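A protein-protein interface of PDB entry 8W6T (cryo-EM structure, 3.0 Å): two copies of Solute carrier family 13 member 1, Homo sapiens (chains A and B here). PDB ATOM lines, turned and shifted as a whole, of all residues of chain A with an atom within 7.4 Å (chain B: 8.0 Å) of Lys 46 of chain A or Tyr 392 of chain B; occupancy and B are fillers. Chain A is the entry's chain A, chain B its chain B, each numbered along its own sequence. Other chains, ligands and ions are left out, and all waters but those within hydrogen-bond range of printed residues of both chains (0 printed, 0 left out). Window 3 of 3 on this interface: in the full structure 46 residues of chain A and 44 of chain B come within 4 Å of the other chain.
Among the printed residues, merely in contact across the chains: Pro 80 of chain A with Phe 395 of chain B (3.3 Å), Gly 83 of chain A with Phe 395 of chain B (3.5 Å), Met 85 of chain A with Phe 395 of chain B (3.7 Å), Gly 83 of chain A with Tyr 392 of chain B (3.7 Å), Met 81 of chain A with Phe 389 of chain B (3.8 Å), Ile 84 of chain A with Phe 395 of chain B (3.9 Å) and Phe 82 of chain A with Tyr 392 of chain B (3.99 Å).
The side-chain carboxylate (OE1) of Glu 49 of chain A is in salt-bridge range of the side-chain amino group (NZ) of Lys 46 of chain A, at 3.6 Å.
NZ of Lys 46 of chain A is in hydrogen-bond range of O of Phe 82 of chain A, at 3.1 Å.
Of chain B, only Tyr 392 comes within 4 Å of Lys 46 of chain A.
Of the printed residues of chain B, Met 81 of chain A touches Phe 389 (3.8 Å).
Of the printed residues of chain B, Met 85 of chain A touches Phe 395 (3.7 Å).
The nearest printed residue of chain B that does not touch Lys 46 of chain A is Phe 395 of chain B (7.1 Å).
The nearest printed residue of chain A that does not touch Tyr 392 of chain B is Pro 80 of chain A (5.6 Å).
Of the 22 printed residues of chain A, 7 touch a printed residue of chain B.
Printed residues of chain A that touch a printed residue of chain B: Lys 46, Pro 80, Met 81, Phe 82, Gly 83, Ile 84 and Met 85.
Hydrophobic or aromatic side chains of chain B that line the printed part of chain A: Phe 389, Tyr 392 and Phe 395.
Among the printed residues, no Asp or Glu carboxylate lies within 4 Å of a Lys or Arg side-chain nitrogen of the other chain.
No position is printed for both chains.
Of the 8 pairs that touch across the chains among the printed residues, none has its exchanged pair printed and touching as well.
The side-chain amino group of Lys 46 of chain A sits at hydrogen-bond distance from the side-chain hydroxyl of Tyr 392 of chain B (2.6 Å).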
ATOM      1  N   LEU A  43     -30.337  17.633  16.797  1.00  0.00           N
ATOM      2  CA  LEU A  43     -31.511  17.878  17.619  1.00  0.00           C
ATOM      3  C   LEU A  43     -31.083  18.608  18.886  1.00  0.00           C
ATOM      4  O   LEU A  43     -30.423  18.028  19.752  1.00  0.00           O
ATOM      5  CB  LEU A  43     -32.203  16.562  17.967  1.00  0.00           C
ATOM      6  CG  LEU A  43     -33.358  16.081  17.087  1.00  0.00           C
ATOM      7  CD1 LEU A  43     -32.880  15.684  15.701  1.00  0.00           C
ATOM      8  CD2 LEU A  43     -34.059  14.919  17.764  1.00  0.00           C
ATOM      9  N   HIS A  44     -31.455  19.882  18.993  1.00  0.00           N
ATOM     10  CA  HIS A  44     -30.950  20.743  20.051  1.00  0.00           C
ATOM     11  C   HIS A  44     -31.782  20.666  21.327  1.00  0.00           C
ATOM     12  O   HIS A  44     -31.410  21.282  22.333  1.00  0.00           O
ATOM     13  CB  HIS A  44     -30.887  22.194  19.533  1.00  0.00           C
ATOM     14  CG  HIS A  44     -30.073  23.122  20.383  1.00  0.00           C
ATOM     15  ND1 HIS A  44     -28.695  23.092  20.408  1.00  0.00           N
ATOM     16  CD2 HIS A  44     -30.443  24.104  21.238  1.00  0.00           C
ATOM     17  CE1 HIS A  44     -28.252  24.016  21.242  1.00  0.00           C
ATOM     18  NE2 HIS A  44     -29.292  24.644  21.758  1.00  0.00           N
ATOM     19  N   THR A  45     -32.857  19.883  21.334  1.00  0.00           N
ATOM     20  CA  THR A  45     -33.740  19.822  22.489  1.00  0.00           C
ATOM     21  C   THR A  45     -33.091  19.046  23.633  1.00  0.00           C
ATOM     22  O   THR A  45     -32.105  18.330  23.454  1.00  0.00           O
ATOM     23  CB  THR A  45     -35.072  19.176  22.110  1.00  0.00           C
ATOM     24  OG1 THR A  45     -34.911  17.755  22.035  1.00  0.00           O
ATOM     25  CG2 THR A  45     -35.543  19.695  20.761  1.00  0.00           C
ATOM     26  N   LYS A  46     -33.664  19.203  24.828  1.00  0.00           N
ATOM     27  CA  LYS A  46     -33.131  18.553  26.019  1.00  0.00           C
ATOM     28  C   LYS A  46     -33.468  17.072  26.084  1.00  0.00           C
ATOM     29  O   LYS A  46     -32.737  16.319  26.739  1.00  0.00           O
ATOM     30  CB  LYS A  46     -33.653  19.247  27.279  1.00  0.00           C
ATOM     31  CG  LYS A  46     -33.333  20.721  27.347  1.00  0.00           C
ATOM     32  CD  LYS A  46     -31.839  20.945  27.398  1.00  0.00           C
ATOM     33  CE  LYS A  46     -31.508  22.422  27.360  1.00  0.00           C
ATOM     34  NZ  LYS A  46     -30.048  22.651  27.208  1.00  0.00           N
ATOM     35  N   GLU A  47     -34.549  16.644  25.426  1.00  0.00           N
ATOM     36  CA  GLU A  47     -34.874  15.224  25.372  1.00  0.00           C
ATOM     37  C   GLU A  47     -33.834  14.448  24.576  1.00  0.00           C
ATOM     38  O   GLU A  47     -33.467  13.335  24.965  1.00  0.00           O
ATOM     39  CB  GLU A  47     -36.261  15.016  24.763  1.00  0.00           C
ATOM     40  CG  GLU A  47     -37.420  15.539  25.600  1.00  0.00           C
ATOM     41  CD  GLU A  47     -37.741  16.996  25.329  1.00  0.00           C
ATOM     42  OE1 GLU A  47     -37.097  17.595  24.445  1.00  0.00           O
ATOM     43  OE2 GLU A  47     -38.647  17.540  25.994  1.00  0.00           O
ATOM     44  N   ALA A  48     -33.324  15.029  23.489  1.00  0.00           N
ATOM     45  CA  ALA A  48     -32.255  14.423  22.706  1.00  0.00           C
ATOM     46  C   ALA A  48     -30.942  14.319  23.469  1.00  0.00           C
ATOM     47  O   ALA A  48     -30.288  13.272  23.404  1.00  0.00           O
ATOM     48  CB  ALA A  48     -32.030  15.221  21.425  1.00  0.00           C
ATOM     49  N   GLU A  49     -30.548  15.366  24.192  1.00  0.00           N
ATOM     50  CA  GLU A  49     -29.343  15.335  25.010  1.00  0.00           C
ATOM     51  C   GLU A  49     -29.453  14.359  26.170  1.00  0.00           C
ATOM     52  O   GLU A  49     -28.485  13.648  26.470  1.00  0.00           O
ATOM     53  CB  GLU A  49     -29.040  16.734  25.548  1.00  0.00           C
ATOM     54  CG  GLU A  49     -28.976  17.798  24.473  1.00  0.00           C
ATOM     55  CD  GLU A  49     -28.847  19.191  25.041  1.00  0.00           C
ATOM     56  OE1 GLU A  49     -28.954  19.339  26.275  1.00  0.00           O
ATOM     57  OE2 GLU A  49     -28.641  20.139  24.257  1.00  0.00           O
ATOM     58  N   CYS A  50     -30.618  14.285  26.812  1.00  0.00           N
ATOM     59  CA  CYS A  50     -30.815  13.298  27.863  1.00  0.00           C
ATOM     60  C   CYS A  50     -30.892  11.877  27.319  1.00  0.00           C
ATOM     61  O   CYS A  50     -30.458  10.946  28.002  1.00  0.00           O
ATOM     62  CB  CYS A  50     -32.076  13.629  28.656  1.00  0.00           C
ATOM     63  SG  CYS A  50     -32.319  12.594  30.101  1.00  0.00           S
ATOM     64  N   ALA A  51     -31.395  11.690  26.093  1.00  0.00           N
ATOM     65  CA  ALA A  51     -31.352  10.373  25.468  1.00  0.00           C
ATOM     66  C   ALA A  51     -29.931   9.973  25.101  1.00  0.00           C
ATOM     67  O   ALA A  51     -29.588   8.791  25.178  1.00  0.00           O
ATOM     68  CB  ALA A  51     -32.246  10.349  24.230  1.00  0.00           C
ATOM     69  N   TYR A  52     -29.100  10.942  24.702  1.00  0.00           N
ATOM     70  CA  TYR A  52     -27.675  10.686  24.495  1.00  0.00           C
ATOM     71  C   TYR A  52     -26.992  10.275  25.794  1.00  0.00           C
ATOM     72  O   TYR A  52     -26.213   9.312  25.815  1.00  0.00           O
ATOM     73  CB  TYR A  52     -27.007  11.932  23.903  1.00  0.00           C
ATOM     74  CG  TYR A  52     -25.498  11.852  23.766  1.00  0.00           C
ATOM     75  CD1 TYR A  52     -24.915  11.218  22.677  1.00  0.00           C
ATOM     76  CD2 TYR A  52     -24.657  12.435  24.712  1.00  0.00           C
ATOM     77  CE1 TYR A  52     -23.543  11.148  22.545  1.00  0.00           C
ATOM     78  CE2 TYR A  52     -23.286  12.362  24.588  1.00  0.00           C
ATOM     79  CZ  TYR A  52     -22.736  11.720  23.501  1.00  0.00           C
ATOM     80  OH  TYR A  52     -21.371  11.651  23.367  1.00  0.00           O
ATOM     81  N   THR A  53     -27.274  11.001  26.882  1.00  0.00           N
ATOM     82  CA  THR A  53     -26.717  10.671  28.193  1.00  0.00           C
ATOM     83  C   THR A  53     -27.186   9.301  28.675  1.00  0.00           C
ATOM     84  O   THR A  53     -26.412   8.551  29.279  1.00  0.00           O
ATOM     85  CB  THR A  53     -27.097  11.756  29.203  1.00  0.00           C
ATOM     86  OG1 THR A  53     -26.814  13.046  28.650  1.00  0.00           O
ATOM     87  CG2 THR A  53     -26.323  11.593  30.503  1.00  0.00           C
ATOM     88  N   PRO A  80     -24.620  18.740  33.876  1.00  0.00           N
ATOM     89  CA  PRO A  80     -24.421  20.198  33.884  1.00  0.00           C
ATOM     90  C   PRO A  80     -23.805  20.736  32.606  1.00  0.00           C
ATOM     91  O   PRO A  80     -24.001  21.916  32.293  1.00  0.00           O
ATOM     92  CB  PRO A  80     -23.494  20.421  35.086  1.00  0.00           C
ATOM     93  CG  PRO A  80     -23.692  19.252  35.933  1.00  0.00           C
ATOM     94  CD  PRO A  80     -23.837  18.138  34.978  1.00  0.00           C
ATOM     95  N   MET A  81     -23.064  19.914  31.859  1.00  0.00           N
ATOM     96  CA  MET A  81     -22.428  20.393  30.637  1.00  0.00           C
ATOM     97  C   MET A  81     -23.410  20.523  29.481  1.00  0.00           C
ATOM     98  O   MET A  81     -23.124  21.246  28.523  1.00  0.00           O
ATOM     99  CB  MET A  81     -21.280  19.466  30.245  1.00  0.00           C
ATOM    100  CG  MET A  81     -20.014  19.688  31.052  1.00  0.00           C
ATOM    101  SD  MET A  81     -18.608  18.745  30.440  1.00  0.00           S
ATOM    102  CE  MET A  81     -18.242  19.631  28.929  1.00  0.00           C
ATOM    103  N   PHE A  82     -24.548  19.838  29.541  1.00  0.00           N
ATOM    104  CA  PHE A  82     -25.603  20.019  28.555  1.00  0.00           C
ATOM    105  C   PHE A  82     -26.596  21.103  28.945  1.00  0.00           C
ATOM    106  O   PHE A  82     -27.293  21.625  28.071  1.00  0.00           O
ATOM    107  CB  PHE A  82     -26.357  18.702  28.330  1.00  0.00           C
ATOM    108  CG  PHE A  82     -25.735  17.814  27.289  1.00  0.00           C
ATOM    109  CD1 PHE A  82     -25.492  18.288  26.012  1.00  0.00           C
ATOM    110  CD2 PHE A  82     -25.412  16.500  27.585  1.00  0.00           C
ATOM    111  CE1 PHE A  82     -24.926  17.473  25.053  1.00  0.00           C
ATOM    112  CE2 PHE A  82     -24.846  15.680  26.630  1.00  0.00           C
ATOM    113  CZ  PHE A  82     -24.604  16.168  25.362  1.00  0.00           C
ATOM    114  N   GLY A  83     -26.670  21.458  30.225  1.00  0.00           N
ATOM    115  CA  GLY A  83     -27.618  22.456  30.676  1.00  0.00           C
ATOM    116  C   GLY A  83     -28.933  21.903  31.168  1.00  0.00           C
ATOM    117  O   GLY A  83     -29.949  22.600  31.095  1.00  0.00           O
ATOM    118  N   ILE A  84     -28.949  20.670  31.669  1.00  0.00           N
ATOM    119  CA  ILE A  84     -30.195  20.062  32.120  1.00  0.00           C
ATOM    120  C   ILE A  84     -30.449  20.385  33.587  1.00  0.00           C
ATOM    121  O   ILE A  84     -31.536  20.845  33.958  1.00  0.00           O
ATOM    122  CB  ILE A  84     -30.165  18.545  31.860  1.00  0.00           C
ATOM    123  CG1 ILE A  84     -30.307  18.265  30.364  1.00  0.00           C
ATOM    124  CG2 ILE A  84     -31.260  17.831  32.636  1.00  0.00           C
ATOM    125  CD1 ILE A  84     -30.140  16.818  29.999  1.00  0.00           C
ATOM    126  N   MET A  85     -29.453  20.167  34.440  1.00  0.00           N
ATOM    127  CA  MET A  85     -29.570  20.498  35.852  1.00  0.00           C
ATOM    128  C   MET A  85     -28.205  20.933  36.358  1.00  0.00           C
ATOM    129  O   MET A  85     -27.183  20.474  35.835  1.00  0.00           O
ATOM    130  CB  MET A  85     -30.104  19.310  36.670  1.00  0.00           C
ATOM    131  CG  MET A  85     -29.283  18.041  36.584  1.00  0.00           C
ATOM    132  SD  MET A  85     -30.210  16.590  37.120  1.00  0.00           S
ATOM    133  CE  MET A  85     -31.034  17.224  38.577  1.00  0.00           C
ATOM    134  N   GLY A 461     -32.478  13.199  36.015  1.00  0.00           N
ATOM    135  CA  GLY A 461     -32.205  13.916  34.785  1.00  0.00           C
ATOM    136  C   GLY A 461     -33.261  13.702  33.719  1.00  0.00           C
ATOM    137  O   GLY A 461     -33.607  14.635  32.989  1.00  0.00           O
ATOM    138  N   GLU A 464     -36.136  15.926  34.869  1.00  0.00           N
ATOM    139  CA  GLU A 464     -35.887  17.354  34.715  1.00  0.00           C
ATOM    140  C   GLU A 464     -35.827  17.773  33.251  1.00  0.00           C
ATOM    141  O   GLU A 464     -36.256  18.882  32.911  1.00  0.00           O
ATOM    142  CB  GLU A 464     -34.588  17.731  35.437  1.00  0.00           C
ATOM    143  CG  GLU A 464     -34.274  19.220  35.474  1.00  0.00           C
ATOM    144  CD  GLU A 464     -35.255  20.010  36.323  1.00  0.00           C
ATOM    145  OE1 GLU A 464     -35.818  19.440  37.280  1.00  0.00           O
ATOM    146  OE2 GLU A 464     -35.468  21.204  36.026  1.00  0.00           O
ATOM    147  N   SER A 465     -35.331  16.905  32.369  1.00  0.00           N
ATOM    148  CA  SER A 465     -35.193  17.277  30.964  1.00  0.00           C
ATOM    149  C   SER A 465     -36.521  17.201  30.220  1.00  0.00           C
ATOM    150  O   SER A 465     -36.828  18.075  29.402  1.00  0.00           O
ATOM    151  CB  SER A 465     -34.159  16.381  30.289  1.00  0.00           C
ATOM    152  OG  SER A 465     -34.545  15.023  30.370  1.00  0.00           O
ATOM    153  N   GLY A 466     -37.319  16.169  30.484  1.00  0.00           N
ATOM    154  CA  GLY A 466     -38.587  15.973  29.810  1.00  0.00           C
ATOM    155  C   GLY A 466     -38.646  14.757  28.913  1.00  0.00           C
ATOM    156  O   GLY A 466     -39.544  14.678  28.068  1.00  0.00           O
ATOM    157  N   LEU A 467     -37.720  13.810  29.061  1.00  0.00           N
ATOM    158  CA  LEU A 467     -37.755  12.608  28.238  1.00  0.00           C
ATOM    159  C   LEU A 467     -38.821  11.632  28.721  1.00  0.00           C
ATOM    160  O   LEU A 467     -39.435  10.929  27.907  1.00  0.00           O
ATOM    161  CB  LEU A 467     -36.375  11.950  28.236  1.00  0.00           C
ATOM    162  CG  LEU A 467     -36.155  10.711  27.372  1.00  0.00           C
ATOM    163  CD1 LEU A 467     -36.463  11.009  25.918  1.00  0.00           C
ATOM    164  CD2 LEU A 467     -34.729  10.230  27.531  1.00  0.00           C
ATOM    165  N   SER B 386     -16.356  30.061  31.108  1.00  0.00           N
ATOM    166  CA  SER B 386     -17.705  30.021  31.653  1.00  0.00           C
ATOM    167  C   SER B 386     -18.673  30.898  30.872  1.00  0.00           C
ATOM    168  O   SER B 386     -19.887  30.768  31.059  1.00  0.00           O
ATOM    169  CB  SER B 386     -17.699  30.445  33.122  1.00  0.00           C
ATOM    170  OG  SER B 386     -17.368  31.814  33.253  1.00  0.00           O
ATOM    171  N   ALA B 387     -18.170  31.782  30.010  1.00  0.00           N
ATOM    172  CA  ALA B 387     -19.001  32.540  29.089  1.00  0.00           C
ATOM    173  C   ALA B 387     -19.338  31.763  27.825  1.00  0.00           C
ATOM    174  O   ALA B 387     -20.162  32.229  27.032  1.00  0.00           O
ATOM    175  CB  ALA B 387     -18.314  33.857  28.711  1.00  0.00           C
ATOM    176  N   LEU B 388     -18.710  30.605  27.610  1.00  0.00           N
ATOM    177  CA  LEU B 388     -19.150  29.712  26.542  1.00  0.00           C
ATOM    178  C   LEU B 388     -20.484  29.070  26.893  1.00  0.00           C
ATOM    179  O   LEU B 388     -21.332  28.862  26.018  1.00  0.00           O
ATOM    180  CB  LEU B 388     -18.092  28.640  26.282  1.00  0.00           C
ATOM    181  CG  LEU B 388     -17.190  28.793  25.058  1.00  0.00           C
ATOM    182  CD1 LEU B 388     -16.385  30.078  25.125  1.00  0.00           C
ATOM    183  CD2 LEU B 388     -16.270  27.592  24.942  1.00  0.00           C
ATOM    184  N   PHE B 389     -20.681  28.749  28.171  1.00  0.00           N
ATOM    185  CA  PHE B 389     -21.954  28.243  28.679  1.00  0.00           C
ATOM    186  C   PHE B 389     -22.721  29.427  29.261  1.00  0.00           C
ATOM    187  O   PHE B 389     -23.081  29.457  30.437  1.00  0.00           O
ATOM    188  CB  PHE B 389     -21.724  27.147  29.716  1.00  0.00           C
ATOM    189  CG  PHE B 389     -20.813  26.045  29.251  1.00  0.00           C
ATOM    190  CD1 PHE B 389     -21.313  24.978  28.522  1.00  0.00           C
ATOM    191  CD2 PHE B 389     -19.460  26.065  29.559  1.00  0.00           C
ATOM    192  CE1 PHE B 389     -20.481  23.958  28.095  1.00  0.00           C
ATOM    193  CE2 PHE B 389     -18.624  25.050  29.135  1.00  0.00           C
ATOM    194  CZ  PHE B 389     -19.135  23.994  28.404  1.00  0.00           C
ATOM    195  N   SER B 390     -22.968  30.422  28.406  1.00  0.00           N
ATOM    196  CA  SER B 390     -23.574  31.671  28.854  1.00  0.00           C
ATOM    197  C   SER B 390     -25.059  31.523  29.151  1.00  0.00           C
ATOM    198  O   SER B 390     -25.619  32.335  29.897  1.00  0.00           O
ATOM    199  CB  SER B 390     -23.363  32.761  27.805  1.00  0.00           C
ATOM    200  OG  SER B 390     -23.996  33.966  28.191  1.00  0.00           O
ATOM    201  N   GLU B 391     -25.713  30.509  28.581  1.00  0.00           N
ATOM    202  CA  GLU B 391     -27.137  30.316  28.824  1.00  0.00           C
ATOM    203  C   GLU B 391     -27.401  29.771  30.220  1.00  0.00           C
ATOM    204  O   GLU B 391     -28.498  29.959  30.760  1.00  0.00           O
ATOM    205  CB  GLU B 391     -27.720  29.372  27.770  1.00  0.00           C
ATOM    206  CG  GLU B 391     -27.518  29.789  26.303  1.00  0.00           C
ATOM    207  CD  GLU B 391     -28.459  30.887  25.795  1.00  0.00           C
ATOM    208  OE1 GLU B 391     -28.741  30.876  24.580  1.00  0.00           O
ATOM    209  OE2 GLU B 391     -28.923  31.751  26.571  1.00  0.00           O
ATOM    210  N   TYR B 392     -26.418  29.097  30.814  1.00  0.00           N
ATOM    211  CA  TYR B 392     -26.560  28.447  32.113  1.00  0.00           C
ATOM    212  C   TYR B 392     -25.414  28.895  33.010  1.00  0.00           C
ATOM    213  O   TYR B 392     -24.298  28.367  32.895  1.00  0.00           O
ATOM    214  CB  TYR B 392     -26.549  26.926  31.946  1.00  0.00           C
ATOM    215  CG  TYR B 392     -27.384  26.453  30.781  1.00  0.00           C
ATOM    216  CD1 TYR B 392     -28.771  26.475  30.842  1.00  0.00           C
ATOM    217  CD2 TYR B 392     -26.783  26.004  29.613  1.00  0.00           C
ATOM    218  CE1 TYR B 392     -29.537  26.049  29.774  1.00  0.00           C
ATOM    219  CE2 TYR B 392     -27.540  25.579  28.540  1.00  0.00           C
ATOM    220  CZ  TYR B 392     -28.915  25.604  28.628  1.00  0.00           C
ATOM    221  OH  TYR B 392     -29.669  25.181  27.559  1.00  0.00           O
ATOM    222  N   PRO B 393     -25.631  29.865  33.908  1.00  0.00           N
ATOM    223  CA  PRO B 393     -24.485  30.491  34.592  1.00  0.00           C
ATOM    224  C   PRO B 393     -23.812  29.616  35.639  1.00  0.00           C
ATOM    225  O   PRO B 393     -22.578  29.530  35.652  1.00  0.00           O
ATOM    226  CB  PRO B 393     -25.103  31.750  35.216  1.00  0.00           C
ATOM    227  CG  PRO B 393     -26.554  31.452  35.332  1.00  0.00           C
ATOM    228  CD  PRO B 393     -26.900  30.556  34.187  1.00  0.00           C
ATOM    229  N   GLY B 394     -24.572  28.963  36.512  1.00  0.00           N
ATOM    230  CA  GLY B 394     -23.959  28.246  37.614  1.00  0.00           C
ATOM    231  C   GLY B 394     -24.105  26.742  37.533  1.00  0.00           C
ATOM    232  O   GLY B 394     -24.188  26.062  38.560  1.00  0.00           O
ATOM    233  N   PHE B 395     -24.122  26.208  36.314  1.00  0.00           N
ATOM    234  CA  PHE B 395     -24.365  24.784  36.107  1.00  0.00           C
ATOM    235  C   PHE B 395     -23.076  23.978  36.239  1.00  0.00           C
ATOM    236  O   PHE B 395     -23.000  23.045  37.044  1.00  0.00           O
ATOM    237  CB  PHE B 395     -25.014  24.557  34.735  1.00  0.00           C
ATOM    238  CG  PHE B 395     -26.518  24.672  34.735  1.00  0.00           C
ATOM    239  CD1 PHE B 395     -27.155  25.750  35.329  1.00  0.00           C
ATOM    240  CD2 PHE B 395     -27.291  23.703  34.122  1.00  0.00           C
ATOM    241  CE1 PHE B 395     -28.532  25.854  35.320  1.00  0.00           C
ATOM    242  CE2 PHE B 395     -28.670  23.800  34.108  1.00  0.00           C
ATOM    243  CZ  PHE B 395     -29.290  24.877  34.708  1.00  0.00           C
ATOM    244  N   ALA B 396     -22.055  24.333  35.463  1.00  0.00           N
ATOM    245  CA  ALA B 396     -20.768  23.639  35.494  1.00  0.00           C
ATOM    246  C   ALA B 396     -19.849  24.365  36.467  1.00  0.00           C
ATOM    247  O   ALA B 396     -19.356  25.461  36.199  1.00  0.00           O
ATOM    248  CB  ALA B 396     -20.162  23.566  34.099  1.00  0.00           C
